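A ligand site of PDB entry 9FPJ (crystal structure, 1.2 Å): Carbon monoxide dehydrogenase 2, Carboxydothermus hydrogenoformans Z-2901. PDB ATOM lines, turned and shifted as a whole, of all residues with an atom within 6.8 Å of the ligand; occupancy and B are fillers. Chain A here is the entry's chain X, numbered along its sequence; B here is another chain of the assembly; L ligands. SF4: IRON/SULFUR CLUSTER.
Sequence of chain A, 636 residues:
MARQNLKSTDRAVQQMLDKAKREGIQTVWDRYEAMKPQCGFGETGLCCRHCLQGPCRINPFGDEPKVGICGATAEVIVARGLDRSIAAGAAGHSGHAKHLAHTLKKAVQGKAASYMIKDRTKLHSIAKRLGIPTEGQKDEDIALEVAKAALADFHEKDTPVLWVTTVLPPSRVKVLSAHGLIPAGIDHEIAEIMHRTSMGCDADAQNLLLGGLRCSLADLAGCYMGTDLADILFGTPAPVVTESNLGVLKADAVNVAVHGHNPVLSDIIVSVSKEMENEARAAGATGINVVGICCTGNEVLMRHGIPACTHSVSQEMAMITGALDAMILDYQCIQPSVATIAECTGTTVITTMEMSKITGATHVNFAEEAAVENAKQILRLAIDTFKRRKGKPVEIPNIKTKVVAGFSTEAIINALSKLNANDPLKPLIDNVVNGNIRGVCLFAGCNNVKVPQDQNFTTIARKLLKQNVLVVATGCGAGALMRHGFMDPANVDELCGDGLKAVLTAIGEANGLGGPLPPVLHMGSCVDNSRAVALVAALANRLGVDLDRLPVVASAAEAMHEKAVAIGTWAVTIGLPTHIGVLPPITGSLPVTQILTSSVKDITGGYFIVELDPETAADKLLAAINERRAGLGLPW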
ATOM      1  N   CYS A  47      29.787   5.019  25.587  1.00  0.00           N
ATOM      2  CA  CYS A  47      29.110   4.018  24.763  1.00  0.00           C
ATOM      3  C   CYS A  47      29.213   2.691  25.506  1.00  0.00           C
ATOM      4  O   CYS A  47      30.263   2.377  26.087  1.00  0.00           O
ATOM      5  CB  CYS A  47      29.745   3.850  23.390  1.00  0.00           C
ATOM      6  SG  CYS A  47      28.903   2.599  22.421  1.00  0.00           S
ATOM      7  N   CYS A  48      28.115   1.925  25.489  1.00  0.00           N
ATOM      8  CA  CYS A  48      28.090   0.601  26.092  1.00  0.00           C
ATOM      9  C   CYS A  48      27.372  -0.343  25.155  1.00  0.00           C
ATOM     10  O   CYS A  48      26.282  -0.034  24.650  1.00  0.00           O
ATOM     11  CB  CYS A  48      27.353   0.644  27.424  1.00  0.00           C
ATOM     12  SG  CYS A  48      27.262  -0.960  28.259  1.00  0.00           S
ATOM     13  N   ARG A  49      27.976  -1.516  24.942  1.00  0.00           N
ATOM     14  CA  ARG A  49      27.412  -2.622  24.170  1.00  0.00           C
ATOM     15  C   ARG A  49      27.421  -3.897  24.994  1.00  0.00           C
ATOM     16  O   ARG A  49      27.565  -5.004  24.467  1.00  0.00           O
ATOM     17  CB  ARG A  49      28.178  -2.790  22.850  1.00  0.00           C
ATOM     18  CG  ARG A  49      28.073  -1.592  21.936  1.00  0.00           C
ATOM     19  CD  ARG A  49      29.080  -1.675  20.814  1.00  0.00           C
ATOM     20  NE  ARG A  49      28.829  -2.858  20.009  1.00  0.00           N
ATOM     21  CZ  ARG A  49      29.703  -3.451  19.223  1.00  0.00           C
ATOM     22  NH1 ARG A  49      30.917  -2.958  19.047  1.00  0.00           N
ATOM     23  NH2 ARG A  49      29.349  -4.543  18.557  1.00  0.00           N
ATOM     24  N   HIS A  50      27.285  -3.774  26.320  1.00  0.00           N
ATOM     25  CA  HIS A  50      27.369  -4.958  27.177  1.00  0.00           C
ATOM     26  C   HIS A  50      26.097  -5.792  27.209  1.00  0.00           C
ATOM     27  O   HIS A  50      26.091  -6.845  27.871  1.00  0.00           O
ATOM     28  CB  HIS A  50      27.826  -4.600  28.580  1.00  0.00           C
ATOM     29  CG  HIS A  50      29.238  -4.086  28.656  1.00  0.00           C
ATOM     30  ND1 HIS A  50      29.941  -4.006  29.842  1.00  0.00           N
ATOM     31  CD2 HIS A  50      30.075  -3.589  27.703  1.00  0.00           C
ATOM     32  CE1 HIS A  50      31.134  -3.500  29.610  1.00  0.00           C
ATOM     33  NE2 HIS A  50      31.248  -3.240  28.323  1.00  0.00           N
ATOM     34  N   CYS A  51      25.037  -5.395  26.527  1.00  0.00           N
ATOM     35  CA  CYS A  51      23.915  -6.309  26.349  1.00  0.00           C
ATOM     36  C   CYS A  51      23.180  -5.997  25.056  1.00  0.00           C
ATOM     37  O   CYS A  51      23.465  -5.010  24.365  1.00  0.00           O
ATOM     38  CB  CYS A  51      22.962  -6.294  27.541  1.00  0.00           C
ATOM     39  SG  CYS A  51      21.740  -4.916  27.540  1.00  0.00           S
ATOM     40  N   LEU A  52      22.229  -6.876  24.714  1.00  0.00           N
ATOM     41  CA  LEU A  52      21.530  -6.775  23.440  1.00  0.00           C
ATOM     42  C   LEU A  52      20.400  -5.744  23.454  1.00  0.00           C
ATOM     43  O   LEU A  52      19.695  -5.608  22.449  1.00  0.00           O
ATOM     44  CB  LEU A  52      21.017  -8.137  22.979  1.00  0.00           C
ATOM     45  CG  LEU A  52      22.097  -9.198  22.797  1.00  0.00           C
ATOM     46  CD1 LEU A  52      21.476 -10.489  22.325  1.00  0.00           C
ATOM     47  CD2 LEU A  52      23.149  -8.722  21.827  1.00  0.00           C
ATOM     48  N   GLN A  53      20.230  -5.006  24.556  1.00  0.00           N
ATOM     49  CA  GLN A  53      19.404  -3.804  24.495  1.00  0.00           C
ATOM     50  C   GLN A  53      20.155  -2.622  23.899  1.00  0.00           C
ATOM     51  O   GLN A  53      19.512  -1.653  23.472  1.00  0.00           O
ATOM     52  CB  GLN A  53      18.839  -3.430  25.876  1.00  0.00           C
ATOM     53  CG  GLN A  53      17.900  -4.506  26.383  1.00  0.00           C
ATOM     54  CD  GLN A  53      17.262  -4.232  27.718  1.00  0.00           C
ATOM     55  OE1 GLN A  53      16.153  -4.713  27.962  1.00  0.00           O
ATOM     56  NE2 GLN A  53      17.940  -3.506  28.608  1.00  0.00           N
ATOM     57  N   GLY A  54      21.479  -2.672  23.882  1.00  0.00           N
ATOM     58  CA  GLY A  54      22.276  -1.631  23.302  1.00  0.00           C
ATOM     59  C   GLY A  54      22.279  -1.703  21.795  1.00  0.00           C
ATOM     60  O   GLY A  54      21.577  -2.499  21.172  1.00  0.00           O
ATOM     61  N   PRO A  55      23.100  -0.882  21.177  1.00  0.00           N
ATOM     62  CA  PRO A  55      24.096  -0.023  21.823  1.00  0.00           C
ATOM     63  C   PRO A  55      23.484   1.161  22.544  1.00  0.00           C
ATOM     64  O   PRO A  55      22.516   1.762  22.072  1.00  0.00           O
ATOM     65  CB  PRO A  55      24.963   0.439  20.656  1.00  0.00           C
ATOM     66  CG  PRO A  55      24.016   0.426  19.477  1.00  0.00           C
ATOM     67  CD  PRO A  55      23.130  -0.762  19.707  1.00  0.00           C
ATOM     68  N   CYS A  56      24.042   1.472  23.708  1.00  0.00           N
ATOM     69  CA  CYS A  56      23.690   2.660  24.470  1.00  0.00           C
ATOM     70  C   CYS A  56      24.798   3.690  24.361  1.00  0.00           C
ATOM     71  O   CYS A  56      25.993   3.346  24.260  1.00  0.00           O
ATOM     72  CB  CYS A  56      23.452   2.296  25.940  1.00  0.00           C
ATOM     73  SG  CYS A  56      21.920   1.354  26.155  1.00  0.00           S
ATOM     74  N   ARG A  57      24.407   4.957  24.445  1.00  0.00           N
ATOM     75  CA  ARG A  57      25.354   6.058  24.490  1.00  0.00           C
ATOM     76  C   ARG A  57      24.785   7.131  25.395  1.00  0.00           C
ATOM     77  O   ARG A  57      23.604   7.148  25.721  1.00  0.00           O
ATOM     78  CB  ARG A  57      25.611   6.601  23.082  1.00  0.00           C
ATOM     79  CG  ARG A  57      24.427   7.341  22.529  1.00  0.00           C
ATOM     80  CD  ARG A  57      24.457   7.514  21.005  1.00  0.00           C
ATOM     81  NE  ARG A  57      23.326   8.309  20.543  1.00  0.00           N
ATOM     82  CZ  ARG A  57      22.075   7.886  20.564  1.00  0.00           C
ATOM     83  NH1 ARG A  57      21.773   6.612  20.742  1.00  0.00           N
ATOM     84  NH2 ARG A  57      21.088   8.768  20.389  1.00  0.00           N
ATOM     85  N   VAL A  67      21.524   8.562  30.179  1.00  0.00           N
ATOM     86  CA  VAL A  67      21.718   7.354  30.982  1.00  0.00           C
ATOM     87  C   VAL A  67      21.465   6.159  30.073  1.00  0.00           C
ATOM     88  O   VAL A  67      20.690   6.234  29.108  1.00  0.00           O
ATOM     89  CB  VAL A  67      20.779   7.405  32.213  1.00  0.00           C
ATOM     90  CG1 VAL A  67      19.328   7.427  31.758  1.00  0.00           C
ATOM     91  CG2 VAL A  67      21.055   6.302  33.188  1.00  0.00           C
ATOM     92  N   GLY A  68      22.146   5.050  30.360  1.00  0.00           N
ATOM     93  CA  GLY A  68      21.915   3.838  29.612  1.00  0.00           C
ATOM     94  C   GLY A  68      20.527   3.278  29.836  1.00  0.00           C
ATOM     95  O   GLY A  68      19.824   3.614  30.794  1.00  0.00           O
ATOM     96  N   ILE A  69      20.127   2.353  28.956  1.00  0.00           N
ATOM     97  CA  ILE A  69      18.770   1.823  29.001  1.00  0.00           C
ATOM     98  C   ILE A  69      18.478   1.131  30.325  1.00  0.00           C
ATOM     99  O   ILE A  69      17.383   1.270  30.898  1.00  0.00           O
ATOM    100  CB  ILE A  69      18.490   0.938  27.783  1.00  0.00           C
ATOM    101  CG1 ILE A  69      18.391   1.811  26.523  1.00  0.00           C
ATOM    102  CG2 ILE A  69      17.214   0.119  27.983  1.00  0.00           C
ATOM    103  CD1 ILE A  69      18.326   1.030  25.221  1.00  0.00           C
ATOM    104  N   CYS A  70      19.448   0.382  30.871  1.00  0.00           N
ATOM    105  CA  CYS A  70      19.261  -0.296  32.158  1.00  0.00           C
ATOM    106  C   CYS A  70      19.396   0.635  33.359  1.00  0.00           C
ATOM    107  O   CYS A  70      19.195   0.180  34.501  1.00  0.00           O
ATOM    108  CB  CYS A  70      20.293  -1.407  32.305  1.00  0.00           C
ATOM    109  SG  CYS A  70      22.003  -0.758  32.262  1.00  0.00           S
ATOM    110  N   GLY A  71      19.719   1.910  33.114  1.00  0.00           N
ATOM    111  CA  GLY A  71      20.024   2.876  34.152  1.00  0.00           C
ATOM    112  C   GLY A  71      21.497   3.120  34.403  1.00  0.00           C
ATOM    113  O   GLY A  71      21.837   3.882  35.308  1.00  0.00           O
ATOM    114  N   ALA A  72      22.389   2.477  33.645  1.00  0.00           N
ATOM    115  CA  ALA A  72      23.803   2.684  33.871  1.00  0.00           C
ATOM    116  C   ALA A  72      24.187   4.142  33.612  1.00  0.00           C
ATOM    117  O   ALA A  72      23.908   4.698  32.543  1.00  0.00           O
ATOM    118  CB  ALA A  72      24.598   1.767  32.942  1.00  0.00           C
ATOM    119  N   ILE A  77      29.337   3.317  33.028  1.00  0.00           N
ATOM    120  CA  ILE A  77      29.706   2.906  31.681  1.00  0.00           C
ATOM    121  C   ILE A  77      31.204   3.110  31.464  1.00  0.00           C
ATOM    122  O   ILE A  77      31.906   2.218  30.978  1.00  0.00           O
ATOM    123  CB  ILE A  77      28.846   3.667  30.659  1.00  0.00           C
ATOM    124  CG1 ILE A  77      27.415   3.111  30.703  1.00  0.00           C
ATOM    125  CG2 ILE A  77      29.417   3.606  29.257  1.00  0.00           C
ATOM    126  CD1 ILE A  77      26.415   3.907  29.880  1.00  0.00           C
ATOM    127  N   ARG A  80      33.253   0.577  33.576  1.00  0.00           N
ATOM    128  CA  ARG A  80      33.150  -0.797  33.083  1.00  0.00           C
ATOM    129  C   ARG A  80      34.004  -1.001  31.834  1.00  0.00           C
ATOM    130  O   ARG A  80      34.668  -2.036  31.689  1.00  0.00           O
ATOM    131  CB  ARG A  80      31.688  -1.172  32.793  1.00  0.00           C
ATOM    132  CG  ARG A  80      30.843  -1.238  34.073  1.00  0.00           C
ATOM    133  CD  ARG A  80      29.488  -1.910  33.837  1.00  0.00           C
ATOM    134  NE  ARG A  80      28.710  -1.282  32.779  1.00  0.00           N
ATOM    135  CZ  ARG A  80      27.419  -1.488  32.613  1.00  0.00           C
ATOM    136  NH1 ARG A  80      26.747  -2.276  33.443  1.00  0.00           N
ATOM    137  NH2 ARG A  80      26.778  -0.911  31.609  1.00  0.00           N
ATOM    138  N   THR A 197      31.478  -6.430  35.276  1.00  0.00           N
ATOM    139  CA  THR A 197      31.185  -5.405  34.282  1.00  0.00           C
ATOM    140  C   THR A 197      30.065  -5.812  33.330  1.00  0.00           C
ATOM    141  O   THR A 197      29.673  -5.003  32.478  1.00  0.00           O
ATOM    142  CB  THR A 197      32.436  -5.063  33.447  1.00  0.00           C
ATOM    143  OG1 THR A 197      32.925  -6.254  32.818  1.00  0.00           O
ATOM    144  CG2 THR A 197      33.508  -4.444  34.352  1.00  0.00           C
ATOM    145  N   SER A 198      29.572  -7.051  33.416  1.00  0.00           N
ATOM    146  CA  SER A 198      28.428  -7.477  32.619  1.00  0.00           C
ATOM    147  C   SER A 198      27.161  -6.797  33.128  1.00  0.00           C
ATOM    148  O   SER A 198      27.124  -6.172  34.187  1.00  0.00           O
ATOM    149  CB  SER A 198      28.312  -8.999  32.570  1.00  0.00           C
ATOM    150  OG  SER A 198      27.840  -9.559  33.780  1.00  0.00           O
ATOM    151  N   MET A 199      26.092  -6.883  32.335  1.00  0.00           N
ATOM    152  CA  MET A 199      24.895  -6.116  32.622  1.00  0.00           C
ATOM    153  C   MET A 199      24.302  -6.482  33.977  1.00  0.00           C
ATOM    154  O   MET A 199      24.229  -7.661  34.354  1.00  0.00           O
ATOM    155  CB  MET A 199      23.866  -6.287  31.488  1.00  0.00           C
ATOM    156  CG  MET A 199      22.545  -5.530  31.688  1.00  0.00           C
ATOM    157  SD  MET A 199      21.421  -6.396  32.801  1.00  0.00           S
ATOM    158  CE  MET A 199      20.591  -5.023  33.622  1.00  0.00           C
ATOM    159  N   GLY A 200      23.915  -5.455  34.731  1.00  0.00           N
ATOM    160  CA  GLY A 200      23.165  -5.679  35.951  1.00  0.00           C
ATOM    161  C   GLY A 200      24.003  -6.175  37.107  1.00  0.00           C
ATOM    162  O   GLY A 200      23.461  -6.818  38.020  1.00  0.00           O
ATOM    163  N   VAL B  28      12.644   1.760  32.282  1.00  0.00           N
ATOM    164  CA  VAL B  28      13.483   1.195  31.232  1.00  0.00           C
ATOM    165  C   VAL B  28      12.920   1.523  29.840  1.00  0.00           C
ATOM    166  O   VAL B  28      13.678   1.788  28.904  1.00  0.00           O
ATOM    167  CB  VAL B  28      13.654  -0.330  31.448  1.00  0.00           C
ATOM    168  CG1 VAL B  28      12.309  -1.068  31.352  1.00  0.00           C
ATOM    169  CG2 VAL B  28      14.680  -0.899  30.495  1.00  0.00           C
ATOM    170  N   MET B  35      16.930   6.742  23.887  1.00  0.00           N
ATOM    171  CA  MET B  35      18.122   6.256  23.202  1.00  0.00           C
ATOM    172  C   MET B  35      17.936   6.173  21.685  1.00  0.00           C
ATOM    173  O   MET B  35      18.916   5.998  20.966  1.00  0.00           O
ATOM    174  CB  MET B  35      18.479   4.866  23.756  1.00  0.00           C
ATOM    175  CG  MET B  35      19.925   4.484  23.517  1.00  0.00           C
ATOM    176  SD  MET B  35      21.115   5.609  24.292  1.00  0.00           S
ATOM    177  CE  MET B  35      20.864   5.202  26.022  1.00  0.00           C
ATOM    178  N   GLN B  38      19.166   4.243  17.874  1.00  0.00           N
ATOM    179  CA  GLN B  38      20.424   3.690  18.353  1.00  0.00           C
ATOM    180  C   GLN B  38      21.447   3.618  17.217  1.00  0.00           C
ATOM    181  O   GLN B  38      21.113   3.598  16.032  1.00  0.00           O
ATOM    182  CB  GLN B  38      20.202   2.306  18.978  1.00  0.00           C
ATOM    183  CG  GLN B  38      19.329   2.384  20.216  1.00  0.00           C
ATOM    184  CD  GLN B  38      19.014   1.033  20.823  1.00  0.00           C
ATOM    185  OE1 GLN B  38      18.087   0.361  20.396  1.00  0.00           O
ATOM    186  NE2 GLN B  38      19.788   0.639  21.833  1.00  0.00           N
ATOM    187  N   PRO B 336      20.459  -1.020  37.312  1.00  0.00           N
ATOM    188  CA  PRO B 336      20.920  -0.136  38.383  1.00  0.00           C
ATOM    189  C   PRO B 336      19.972   1.026  38.643  1.00  0.00           C
ATOM    190  O   PRO B 336      20.087   1.688  39.680  1.00  0.00           O
ATOM    191  CB  PRO B 336      22.313   0.291  37.923  1.00  0.00           C
ATOM    192  CG  PRO B 336      22.293   0.129  36.421  1.00  0.00           C
ATOM    193  CD  PRO B 336      21.444  -1.099  36.210  1.00  0.00           C
ATOM    194  N   MET B 560      18.752 -10.850  25.990  1.00  0.00           N
ATOM    195  CA  MET B 560      19.363  -9.583  26.383  1.00  0.00           C
ATOM    196  C   MET B 560      20.804  -9.725  26.848  1.00  0.00           C
ATOM    197  O   MET B 560      21.710  -9.060  26.323  1.00  0.00           O
ATOM    198  CB  MET B 560      18.502  -8.900  27.461  1.00  0.00           C
ATOM    199  CG  MET B 560      19.034  -7.572  28.009  1.00  0.00           C
ATOM    200  SD  MET B 560      20.076  -7.722  29.483  1.00  0.00           S
ATOM    201  CE  MET B 560      18.905  -8.415  30.662  1.00  0.00           C
HETATM  202 FE1  SF4 L   1      22.689  -0.385  27.527  1.00  0.00          FE
HETATM  203 FE2  SF4 L   1      22.905  -3.000  28.067  1.00  0.00          FE
HETATM  204 FE3  SF4 L   1      24.979  -1.350  28.452  1.00  0.00          FE
HETATM  205 FE4  SF4 L   1      22.865  -1.163  30.126  1.00  0.00          FE
HETATM  206  S1  SF4 L   1      24.344  -2.950  29.873  1.00  0.00           S
HETATM  207  S2  SF4 L   1      23.987   0.533  29.197  1.00  0.00           S
HETATM  208  S3  SF4 L   1      21.159  -1.578  28.635  1.00  0.00           S
HETATM  209  S4  SF4 L   1      24.039  -1.896  26.432  1.00  0.00           S
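Residues that only touch the ligand: Met 199 (3.6 Å), Ile 69 (3.8 Å), Gly 68 (3.9 Å) and Ala 72 (3.99 Å).
12 residues have an atom within 4 Å of the ligand: Cys 48, His 50, Cys 51, Gln 53, Gly 54, Cys 56, Gly 68, Ile 69, Cys 70, Ala 72, Arg 80 and Met 199.
The nearest printed residue that does not touch the ligand is Arg 49 (4.1 Å).
The backbone NH (N) of Gln 53 sits close to the side-chain sulfur (SG) of Cys 51, at 3.3 Å.
The backbone NH (N) of Cys 48 sits at hydrogen-bond distance from the backbone carbonyl oxygen (O) of Cys 56 (2.8 Å).
SG of Cys 48 lies close to NH2 of Arg 80.
The backbone NH of His 50 lies close to the side-chain sulfur of Cys 48 (3.4 Å).
SG of Cys 70 sits close to N of Ala 72 (3.5 Å).
The backbone NH of Ile 69 lies close to the side-chain sulfur of Cys 56, at 3.5 Å.
A ring nitrogen (ND1) of His 50 is in hydrogen-bond range of the backbone carbonyl oxygen (O) of Thr 197.
The backbone carbonyl oxygen (O) of Gln 53 lies within hydrogen-bond range of the side-chain amide nitrogen (NE2) of Gln 38 of chain B (2.8 Å).
S4 of the ligand sits close to N of Cys 51 (3.6 Å).
FE2 of the ligand is bound by SG of Cys 51 (2.3 Å).
An iron atom (FE3) of the ligand is bound by the side-chain sulfur (SG) of Cys 48 (2.3 Å).
A sulfur (S3) of the ligand sits close to the backbone NH (N) of Cys 70 (3.4 Å).
SG of Cys 70 is bound to FE4 of the ligand.
The side-chain sulfur (SG) of Cys 56 is bound to an iron atom (FE1) of the ligand.
N of Gly 54 sits close to S4 of the ligand (3.7 Å).
The guanidinium group (NH2) of Arg 80 lies close to a sulfur (S1) of the ligand, at 3.6 Å.
A sulfur (S4) of the ligand sits close to the backbone NH (N) of His 50 (3.8 Å).
NE2 of Gln 53 lies close to S3 of the ligand (3.8 Å).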
